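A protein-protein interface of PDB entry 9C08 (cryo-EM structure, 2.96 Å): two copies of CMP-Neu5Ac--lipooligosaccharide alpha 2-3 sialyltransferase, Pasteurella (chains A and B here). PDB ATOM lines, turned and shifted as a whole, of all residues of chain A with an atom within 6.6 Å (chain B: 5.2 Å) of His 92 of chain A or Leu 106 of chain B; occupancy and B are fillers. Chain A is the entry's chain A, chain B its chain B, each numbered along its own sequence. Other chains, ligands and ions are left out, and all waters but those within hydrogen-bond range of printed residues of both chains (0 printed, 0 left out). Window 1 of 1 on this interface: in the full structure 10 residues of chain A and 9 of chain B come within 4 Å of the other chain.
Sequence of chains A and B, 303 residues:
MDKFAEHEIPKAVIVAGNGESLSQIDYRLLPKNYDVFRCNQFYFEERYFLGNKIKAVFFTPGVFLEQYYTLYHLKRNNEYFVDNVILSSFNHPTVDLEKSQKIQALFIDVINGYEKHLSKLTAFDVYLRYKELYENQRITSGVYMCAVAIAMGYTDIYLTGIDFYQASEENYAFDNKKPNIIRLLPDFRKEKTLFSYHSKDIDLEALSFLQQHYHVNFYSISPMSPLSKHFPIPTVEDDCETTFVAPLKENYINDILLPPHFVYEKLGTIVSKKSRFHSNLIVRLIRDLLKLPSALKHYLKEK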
ATOM      1  N   SER A  89      -5.113 -32.249  -3.801  1.00  0.00           N
ATOM      2  CA  SER A  89      -6.170 -31.522  -4.485  1.00  0.00           C
ATOM      3  C   SER A  89      -7.512 -32.209  -4.270  1.00  0.00           C
ATOM      4  O   SER A  89      -7.610 -33.438  -4.292  1.00  0.00           O
ATOM      5  CB  SER A  89      -5.882 -31.413  -5.984  1.00  0.00           C
ATOM      6  OG  SER A  89      -5.839 -32.694  -6.588  1.00  0.00           O
ATOM      7  N   PHE A  90      -8.550 -31.398  -4.058  1.00  0.00           N
ATOM      8  CA  PHE A  90      -9.907 -31.901  -3.908  1.00  0.00           C
ATOM      9  C   PHE A  90     -10.679 -31.947  -5.220  1.00  0.00           C
ATOM     10  O   PHE A  90     -11.780 -32.507  -5.248  1.00  0.00           O
ATOM     11  CB  PHE A  90     -10.686 -31.043  -2.901  1.00  0.00           C
ATOM     12  CG  PHE A  90     -10.146 -31.108  -1.502  1.00  0.00           C
ATOM     13  CD1 PHE A  90     -10.437 -32.186  -0.684  1.00  0.00           C
ATOM     14  CD2 PHE A  90      -9.358 -30.086  -1.001  1.00  0.00           C
ATOM     15  CE1 PHE A  90      -9.945 -32.247   0.605  1.00  0.00           C
ATOM     16  CE2 PHE A  90      -8.865 -30.142   0.288  1.00  0.00           C
ATOM     17  CZ  PHE A  90      -9.158 -31.223   1.090  1.00  0.00           C
ATOM     18  N   ASN A  91     -10.127 -31.382  -6.296  1.00  0.00           N
ATOM     19  CA  ASN A  91     -10.800 -31.316  -7.595  1.00  0.00           C
ATOM     20  C   ASN A  91     -12.182 -30.679  -7.477  1.00  0.00           C
ATOM     21  O   ASN A  91     -13.148 -31.109  -8.111  1.00  0.00           O
ATOM     22  CB  ASN A  91     -10.890 -32.698  -8.244  1.00  0.00           C
ATOM     23  CG  ASN A  91      -9.623 -33.077  -8.981  1.00  0.00           C
ATOM     24  OD1 ASN A  91      -8.568 -32.479  -8.771  1.00  0.00           O
ATOM     25  ND2 ASN A  91      -9.721 -34.073  -9.852  1.00  0.00           N
ATOM     26  N   HIS A  92     -12.277 -29.641  -6.651  1.00  0.00           N
ATOM     27  CA  HIS A  92     -13.537 -28.921  -6.552  1.00  0.00           C
ATOM     28  C   HIS A  92     -13.476 -27.648  -7.385  1.00  0.00           C
ATOM     29  O   HIS A  92     -12.458 -26.947  -7.369  1.00  0.00           O
ATOM     30  CB  HIS A  92     -13.850 -28.570  -5.097  1.00  0.00           C
ATOM     31  CG  HIS A  92     -15.287 -28.232  -4.848  1.00  0.00           C
ATOM     32  ND1 HIS A  92     -15.761 -26.939  -4.856  1.00  0.00           N
ATOM     33  CD2 HIS A  92     -16.355 -29.022  -4.584  1.00  0.00           C
ATOM     34  CE1 HIS A  92     -17.058 -26.945  -4.609  1.00  0.00           C
ATOM     35  NE2 HIS A  92     -17.444 -28.197  -4.440  1.00  0.00           N
ATOM     36  N   PRO A  93     -14.541 -27.335  -8.127  1.00  0.00           N
ATOM     37  CA  PRO A  93     -14.477 -26.203  -9.066  1.00  0.00           C
ATOM     38  C   PRO A  93     -14.218 -24.858  -8.410  1.00  0.00           C
ATOM     39  O   PRO A  93     -13.748 -23.939  -9.092  1.00  0.00           O
ATOM     40  CB  PRO A  93     -15.854 -26.233  -9.744  1.00  0.00           C
ATOM     41  CG  PRO A  93     -16.329 -27.637  -9.577  1.00  0.00           C
ATOM     42  CD  PRO A  93     -15.804 -28.081  -8.247  1.00  0.00           C
ATOM     43  N   THR A  94     -14.506 -24.703  -7.121  1.00  0.00           N
ATOM     44  CA  THR A  94     -14.413 -23.407  -6.465  1.00  0.00           C
ATOM     45  C   THR A  94     -13.084 -23.169  -5.758  1.00  0.00           C
ATOM     46  O   THR A  94     -12.882 -22.080  -5.214  1.00  0.00           O
ATOM     47  CB  THR A  94     -15.558 -23.241  -5.460  1.00  0.00           C
ATOM     48  OG1 THR A  94     -15.496 -24.287  -4.484  1.00  0.00           O
ATOM     49  CG2 THR A  94     -16.901 -23.296  -6.171  1.00  0.00           C
ATOM     50  N   VAL A  95     -12.175 -24.145  -5.740  1.00  0.00           N
ATOM     51  CA  VAL A  95     -10.908 -23.938  -5.045  1.00  0.00           C
ATOM     52  C   VAL A  95      -9.705 -24.171  -5.954  1.00  0.00           C
ATOM     53  O   VAL A  95      -8.936 -23.241  -6.224  1.00  0.00           O
ATOM     54  CB  VAL A  95     -10.823 -24.822  -3.786  1.00  0.00           C
ATOM     55  CG1 VAL A  95     -11.511 -24.137  -2.623  1.00  0.00           C
ATOM     56  CG2 VAL A  95     -11.456 -26.175  -4.035  1.00  0.00           C
ATOM     57  N   ASP A  96      -9.524 -25.406  -6.435  1.00  0.00           N
ATOM     58  CA  ASP A  96      -8.278 -25.762  -7.106  1.00  0.00           C
ATOM     59  C   ASP A  96      -8.494 -26.692  -8.297  1.00  0.00           C
ATOM     60  O   ASP A  96      -7.646 -27.547  -8.575  1.00  0.00           O
ATOM     61  CB  ASP A  96      -7.297 -26.404  -6.122  1.00  0.00           C
ATOM     62  CG  ASP A  96      -7.913 -27.558  -5.353  1.00  0.00           C
ATOM     63  OD1 ASP A  96      -9.098 -27.870  -5.589  1.00  0.00           O
ATOM     64  OD2 ASP A  96      -7.211 -28.153  -4.508  1.00  0.00           O
ATOM     65  N   LEU A  97      -9.616 -26.554  -9.006  1.00  0.00           N
ATOM     66  CA  LEU A  97      -9.870 -27.446 -10.133  1.00  0.00           C
ATOM     67  C   LEU A  97      -8.954 -27.138 -11.313  1.00  0.00           C
ATOM     68  O   LEU A  97      -8.373 -28.054 -11.908  1.00  0.00           O
ATOM     69  CB  LEU A  97     -11.334 -27.354 -10.559  1.00  0.00           C
ATOM     70  CG  LEU A  97     -11.731 -28.239 -11.742  1.00  0.00           C
ATOM     71  CD1 LEU A  97     -11.444 -29.699 -11.439  1.00  0.00           C
ATOM     72  CD2 LEU A  97     -13.195 -28.042 -12.097  1.00  0.00           C
ATOM     73  N   GLU A  98      -8.812 -25.861 -11.669  1.00  0.00           N
ATOM     74  CA  GLU A  98      -7.999 -25.493 -12.824  1.00  0.00           C
ATOM     75  C   GLU A  98      -6.508 -25.546 -12.509  1.00  0.00           C
ATOM     76  O   GLU A  98      -5.699 -25.918 -13.369  1.00  0.00           O
ATOM     77  CB  GLU A  98      -8.392 -24.099 -13.313  1.00  0.00           C
ATOM     78  CG  GLU A  98      -7.786 -23.713 -14.648  1.00  0.00           C
ATOM     79  CD  GLU A  98      -8.238 -22.346 -15.119  1.00  0.00           C
ATOM     80  OE1 GLU A  98      -8.923 -21.645 -14.345  1.00  0.00           O
ATOM     81  OE2 GLU A  98      -7.910 -21.972 -16.264  1.00  0.00           O
ATOM     82  N   LEU A 128     -17.605 -34.020   2.593  1.00  0.00           N
ATOM     83  CA  LEU A 128     -16.660 -32.927   2.396  1.00  0.00           C
ATOM     84  C   LEU A 128     -17.167 -31.924   1.371  1.00  0.00           C
ATOM     85  O   LEU A 128     -17.037 -30.711   1.570  1.00  0.00           O
ATOM     86  CB  LEU A 128     -15.298 -33.474   1.971  1.00  0.00           C
ATOM     87  CG  LEU A 128     -14.468 -34.192   3.031  1.00  0.00           C
ATOM     88  CD1 LEU A 128     -13.062 -34.427   2.509  1.00  0.00           C
ATOM     89  CD2 LEU A 128     -14.440 -33.396   4.326  1.00  0.00           C
ATOM     90  N   ARG A 129     -17.736 -32.404   0.261  1.00  0.00           N
ATOM     91  CA  ARG A 129     -18.226 -31.488  -0.764  1.00  0.00           C
ATOM     92  C   ARG A 129     -19.378 -30.636  -0.255  1.00  0.00           C
ATOM     93  O   ARG A 129     -19.421 -29.431  -0.530  1.00  0.00           O
ATOM     94  CB  ARG A 129     -18.643 -32.263  -2.014  1.00  0.00           C
ATOM     95  CG  ARG A 129     -17.490 -32.960  -2.716  1.00  0.00           C
ATOM     96  CD  ARG A 129     -17.944 -33.681  -3.973  1.00  0.00           C
ATOM     97  NE  ARG A 129     -17.922 -32.809  -5.140  1.00  0.00           N
ATOM     98  CZ  ARG A 129     -16.884 -32.681  -5.956  1.00  0.00           C
ATOM     99  NH1 ARG A 129     -15.763 -33.353  -5.760  1.00  0.00           N
ATOM    100  NH2 ARG A 129     -16.975 -31.857  -6.995  1.00  0.00           N
ATOM    101  N   TYR A 130     -20.313 -31.229   0.494  1.00  0.00           N
ATOM    102  CA  TYR A 130     -21.405 -30.438   1.053  1.00  0.00           C
ATOM    103  C   TYR A 130     -20.880 -29.387   2.022  1.00  0.00           C
ATOM    104  O   TYR A 130     -21.289 -28.221   1.970  1.00  0.00           O
ATOM    105  CB  TYR A 130     -22.422 -31.339   1.750  1.00  0.00           C
ATOM    106  CG  TYR A 130     -23.456 -30.556   2.529  1.00  0.00           C
ATOM    107  CD1 TYR A 130     -24.552 -29.992   1.892  1.00  0.00           C
ATOM    108  CD2 TYR A 130     -23.327 -30.368   3.899  1.00  0.00           C
ATOM    109  CE1 TYR A 130     -25.493 -29.270   2.597  1.00  0.00           C
ATOM    110  CE2 TYR A 130     -24.262 -29.647   4.612  1.00  0.00           C
ATOM    111  CZ  TYR A 130     -25.343 -29.100   3.956  1.00  0.00           C
ATOM    112  OH  TYR A 130     -26.279 -28.383   4.662  1.00  0.00           O
ATOM    113  N   GLU A 132     -17.935 -28.026   2.139  1.00  0.00           N
ATOM    114  CA  GLU A 132     -17.202 -26.997   1.411  1.00  0.00           C
ATOM    115  C   GLU A 132     -18.147 -26.038   0.701  1.00  0.00           C
ATOM    116  O   GLU A 132     -17.957 -24.817   0.750  1.00  0.00           O
ATOM    117  CB  GLU A 132     -16.247 -27.644   0.409  1.00  0.00           C
ATOM    118  CG  GLU A 132     -15.561 -26.660  -0.527  1.00  0.00           C
ATOM    119  CD  GLU A 132     -14.557 -25.771   0.182  1.00  0.00           C
ATOM    120  OE1 GLU A 132     -14.036 -26.182   1.241  1.00  0.00           O
ATOM    121  OE2 GLU A 132     -14.288 -24.660  -0.319  1.00  0.00           O
ATOM    122  N   LEU A 133     -19.176 -26.568   0.039  1.00  0.00           N
ATOM    123  CA  LEU A 133     -20.064 -25.728  -0.755  1.00  0.00           C
ATOM    124  C   LEU A 133     -20.990 -24.863   0.092  1.00  0.00           C
ATOM    125  O   LEU A 133     -21.149 -23.672  -0.198  1.00  0.00           O
ATOM    126  CB  LEU A 133     -20.899 -26.593  -1.704  1.00  0.00           C
ATOM    127  CG  LEU A 133     -21.894 -25.846  -2.594  1.00  0.00           C
ATOM    128  CD1 LEU A 133     -21.182 -24.809  -3.443  1.00  0.00           C
ATOM    129  CD2 LEU A 133     -22.666 -26.818  -3.471  1.00  0.00           C
ATOM    130  N   LEU B  65     -29.840 -25.715  -6.345  1.00  0.00           N
ATOM    131  CA  LEU B  65     -29.088 -25.466  -5.121  1.00  0.00           C
ATOM    132  C   LEU B  65     -30.007 -25.282  -3.921  1.00  0.00           C
ATOM    133  O   LEU B  65     -29.687 -25.744  -2.821  1.00  0.00           O
ATOM    134  CB  LEU B  65     -28.184 -24.243  -5.291  1.00  0.00           C
ATOM    135  CG  LEU B  65     -26.786 -24.483  -5.869  1.00  0.00           C
ATOM    136  CD1 LEU B  65     -26.850 -24.956  -7.314  1.00  0.00           C
ATOM    137  CD2 LEU B  65     -25.935 -23.228  -5.747  1.00  0.00           C
ATOM    138  N   LYS B 102     -22.580 -27.837 -15.226  1.00  0.00           N
ATOM    139  CA  LYS B 102     -22.204 -27.080 -14.034  1.00  0.00           C
ATOM    140  C   LYS B 102     -22.696 -27.766 -12.765  1.00  0.00           C
ATOM    141  O   LYS B 102     -21.971 -27.833 -11.766  1.00  0.00           O
ATOM    142  CB  LYS B 102     -22.751 -25.656 -14.115  1.00  0.00           C
ATOM    143  CG  LYS B 102     -21.941 -24.724 -14.997  1.00  0.00           C
ATOM    144  CD  LYS B 102     -22.477 -23.304 -14.918  1.00  0.00           C
ATOM    145  CE  LYS B 102     -21.546 -22.322 -15.606  1.00  0.00           C
ATOM    146  NZ  LYS B 102     -21.345 -22.656 -17.040  1.00  0.00           N
ATOM    147  N   ILE B 103     -23.930 -28.274 -12.782  1.00  0.00           N
ATOM    148  CA  ILE B 103     -24.468 -28.961 -11.610  1.00  0.00           C
ATOM    149  C   ILE B 103     -23.704 -30.253 -11.347  1.00  0.00           C
ATOM    150  O   ILE B 103     -23.364 -30.566 -10.199  1.00  0.00           O
ATOM    151  CB  ILE B 103     -25.976 -29.218 -11.785  1.00  0.00           C
ATOM    152  CG1 ILE B 103     -26.749 -27.898 -11.741  1.00  0.00           C
ATOM    153  CG2 ILE B 103     -26.486 -30.168 -10.715  1.00  0.00           C
ATOM    154  CD1 ILE B 103     -28.237 -28.056 -11.944  1.00  0.00           C
ATOM    155  N   GLN B 104     -23.419 -31.024 -12.400  1.00  0.00           N
ATOM    156  CA  GLN B 104     -22.718 -32.291 -12.221  1.00  0.00           C
ATOM    157  C   GLN B 104     -21.270 -32.103 -11.790  1.00  0.00           C
ATOM    158  O   GLN B 104     -20.695 -33.017 -11.189  1.00  0.00           O
ATOM    159  CB  GLN B 104     -22.774 -33.111 -13.510  1.00  0.00           C
ATOM    160  CG  GLN B 104     -24.166 -33.600 -13.875  1.00  0.00           C
ATOM    161  CD  GLN B 104     -24.179 -34.427 -15.144  1.00  0.00           C
ATOM    162  OE1 GLN B 104     -25.183 -34.480 -15.853  1.00  0.00           O
ATOM    163  NE2 GLN B 104     -23.062 -35.082 -15.435  1.00  0.00           N
ATOM    164  N   ALA B 105     -20.666 -30.951 -12.084  1.00  0.00           N
ATOM    165  CA  ALA B 105     -19.305 -30.695 -11.629  1.00  0.00           C
ATOM    166  C   ALA B 105     -19.222 -30.429 -10.131  1.00  0.00           C
ATOM    167  O   ALA B 105     -18.128 -30.510  -9.562  1.00  0.00           O
ATOM    168  CB  ALA B 105     -18.707 -29.512 -12.393  1.00  0.00           C
ATOM    169  N   LEU B 106     -20.344 -30.120  -9.481  1.00  0.00           N
ATOM    170  CA  LEU B 106     -20.372 -29.814  -8.055  1.00  0.00           C
ATOM    171  C   LEU B 106     -20.747 -31.009  -7.190  1.00  0.00           C
ATOM    172  O   LEU B 106     -20.212 -31.158  -6.087  1.00  0.00           O
ATOM    173  CB  LEU B 106     -21.353 -28.670  -7.778  1.00  0.00           C
ATOM    174  CG  LEU B 106     -20.966 -27.273  -8.265  1.00  0.00           C
ATOM    175  CD1 LEU B 106     -22.110 -26.300  -8.041  1.00  0.00           C
ATOM    176  CD2 LEU B 106     -19.711 -26.793  -7.559  1.00  0.00           C
ATOM    177  N   PHE B 107     -21.653 -31.862  -7.657  1.00  0.00           N
ATOM    178  CA  PHE B 107     -22.141 -32.992  -6.883  1.00  0.00           C
ATOM    179  C   PHE B 107     -21.768 -34.299  -7.572  1.00  0.00           C
ATOM    180  O   PHE B 107     -21.635 -34.364  -8.796  1.00  0.00           O
ATOM    181  CB  PHE B 107     -23.663 -32.919  -6.692  1.00  0.00           C
ATOM    182  CG  PHE B 107     -24.153 -31.576  -6.234  1.00  0.00           C
ATOM    183  CD1 PHE B 107     -24.048 -31.201  -4.906  1.00  0.00           C
ATOM    184  CD2 PHE B 107     -24.721 -30.688  -7.130  1.00  0.00           C
ATOM    185  CE1 PHE B 107     -24.498 -29.966  -4.484  1.00  0.00           C
ATOM    186  CE2 PHE B 107     -25.174 -29.453  -6.713  1.00  0.00           C
ATOM    187  CZ  PHE B 107     -25.061 -29.091  -5.389  1.00  0.00           C
ATOM    188  N   ILE B 108     -21.598 -35.343  -6.764  1.00  0.00           N
ATOM    189  CA  ILE B 108     -21.233 -36.661  -7.270  1.00  0.00           C
ATOM    190  C   ILE B 108     -22.323 -37.700  -7.065  1.00  0.00           C
ATOM    191  O   ILE B 108     -22.257 -38.772  -7.688  1.00  0.00           O
ATOM    192  CB  ILE B 108     -19.913 -37.160  -6.644  1.00  0.00           C
ATOM    193  CG1 ILE B 108     -20.085 -37.363  -5.137  1.00  0.00           C
ATOM    194  CG2 ILE B 108     -18.785 -36.183  -6.932  1.00  0.00           C
ATOM    195  CD1 ILE B 108     -18.870 -37.944  -4.459  1.00  0.00           C
ATOM    196  N   LEU B 267     -20.110 -18.672  -6.481  1.00  0.00           N
ATOM    197  CA  LEU B 267     -20.562 -19.188  -7.767  1.00  0.00           C
ATOM    198  C   LEU B 267     -20.604 -18.121  -8.851  1.00  0.00           C
ATOM    199  O   LEU B 267     -20.871 -18.449 -10.012  1.00  0.00           O
ATOM    200  CB  LEU B 267     -21.947 -19.830  -7.628  1.00  0.00           C
ATOM    201  CG  LEU B 267     -22.015 -21.326  -7.307  1.00  0.00           C
ATOM    202  CD1 LEU B 267     -21.183 -22.127  -8.297  1.00  0.00           C
ATOM    203  CD2 LEU B 267     -21.582 -21.614  -5.881  1.00  0.00           C
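No position is printed for both chains.
The backbone carbonyl oxygen (O) of Ala 105 of chain B lies within hydrogen-bond range of the guanidinium group (NH2) of Arg 129 of chain A (3.1 Å).
O of Leu 106 of chain B sits at hydrogen-bond distance from NE of Arg 129 of chain A, 3.0 Å away.
Among the printed residues, merely in contact across the chains: Pro 93 of chain A with Ala 105 of chain B, Leu 133 of chain A with Phe 107 of chain B, Arg 129 of chain A with Ile 108 of chain B and His 92 of chain A with Leu 106 of chain B.
Of the 9 printed residues of chain B, 4 touch a printed residue of chain A.
Printed residues of chain B that touch a printed residue of chain A: Ala 105, Leu 106, Phe 107 and Ile 108.
Hydrophobic or aromatic side chains of chain B within 4 Å of the printed part of chain A: Leu 106, Phe 107 and Ile 108.
Of the 15 printed residues of chain A, 4 touch a printed residue of chain B.
Hydrophobic or aromatic side chains of chain A within 4 Å of the printed part of chain B: His 92, Pro 93 and Leu 133.
Among the printed residues, 6 pairs touch across the chains.
OG1 of Thr 94 of chain A sits at hydrogen-bond distance from ND1 of His 92 of chain A (2.7 Å).
The backbone NH (N) of Leu 97 of chain A is in hydrogen-bond range of the backbone carbonyl oxygen (O) of His 92 of chain A.
Asn 91 of chain A touches none of the printed residues of chain B.
Of chain B, only Leu 106 (3.97 Å) comes within 4 Å of His 92 of chain A.
Printed residues of chain B within 4 Å of Pro 93 of chain A: Ala 105.
Printed residues of chain A within 4 Å of Ala 105 of chain B: Pro 93 (3.4 Å) and Arg 129 (3.1 Å).
Leu 106 of chain B touches two residues of chain A.
Of the printed residues of chain A, Ile 108 of chain B touches Arg 129 (3.9 Å).
Leu 267 of chain B touches none of the printed residues of chain A.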
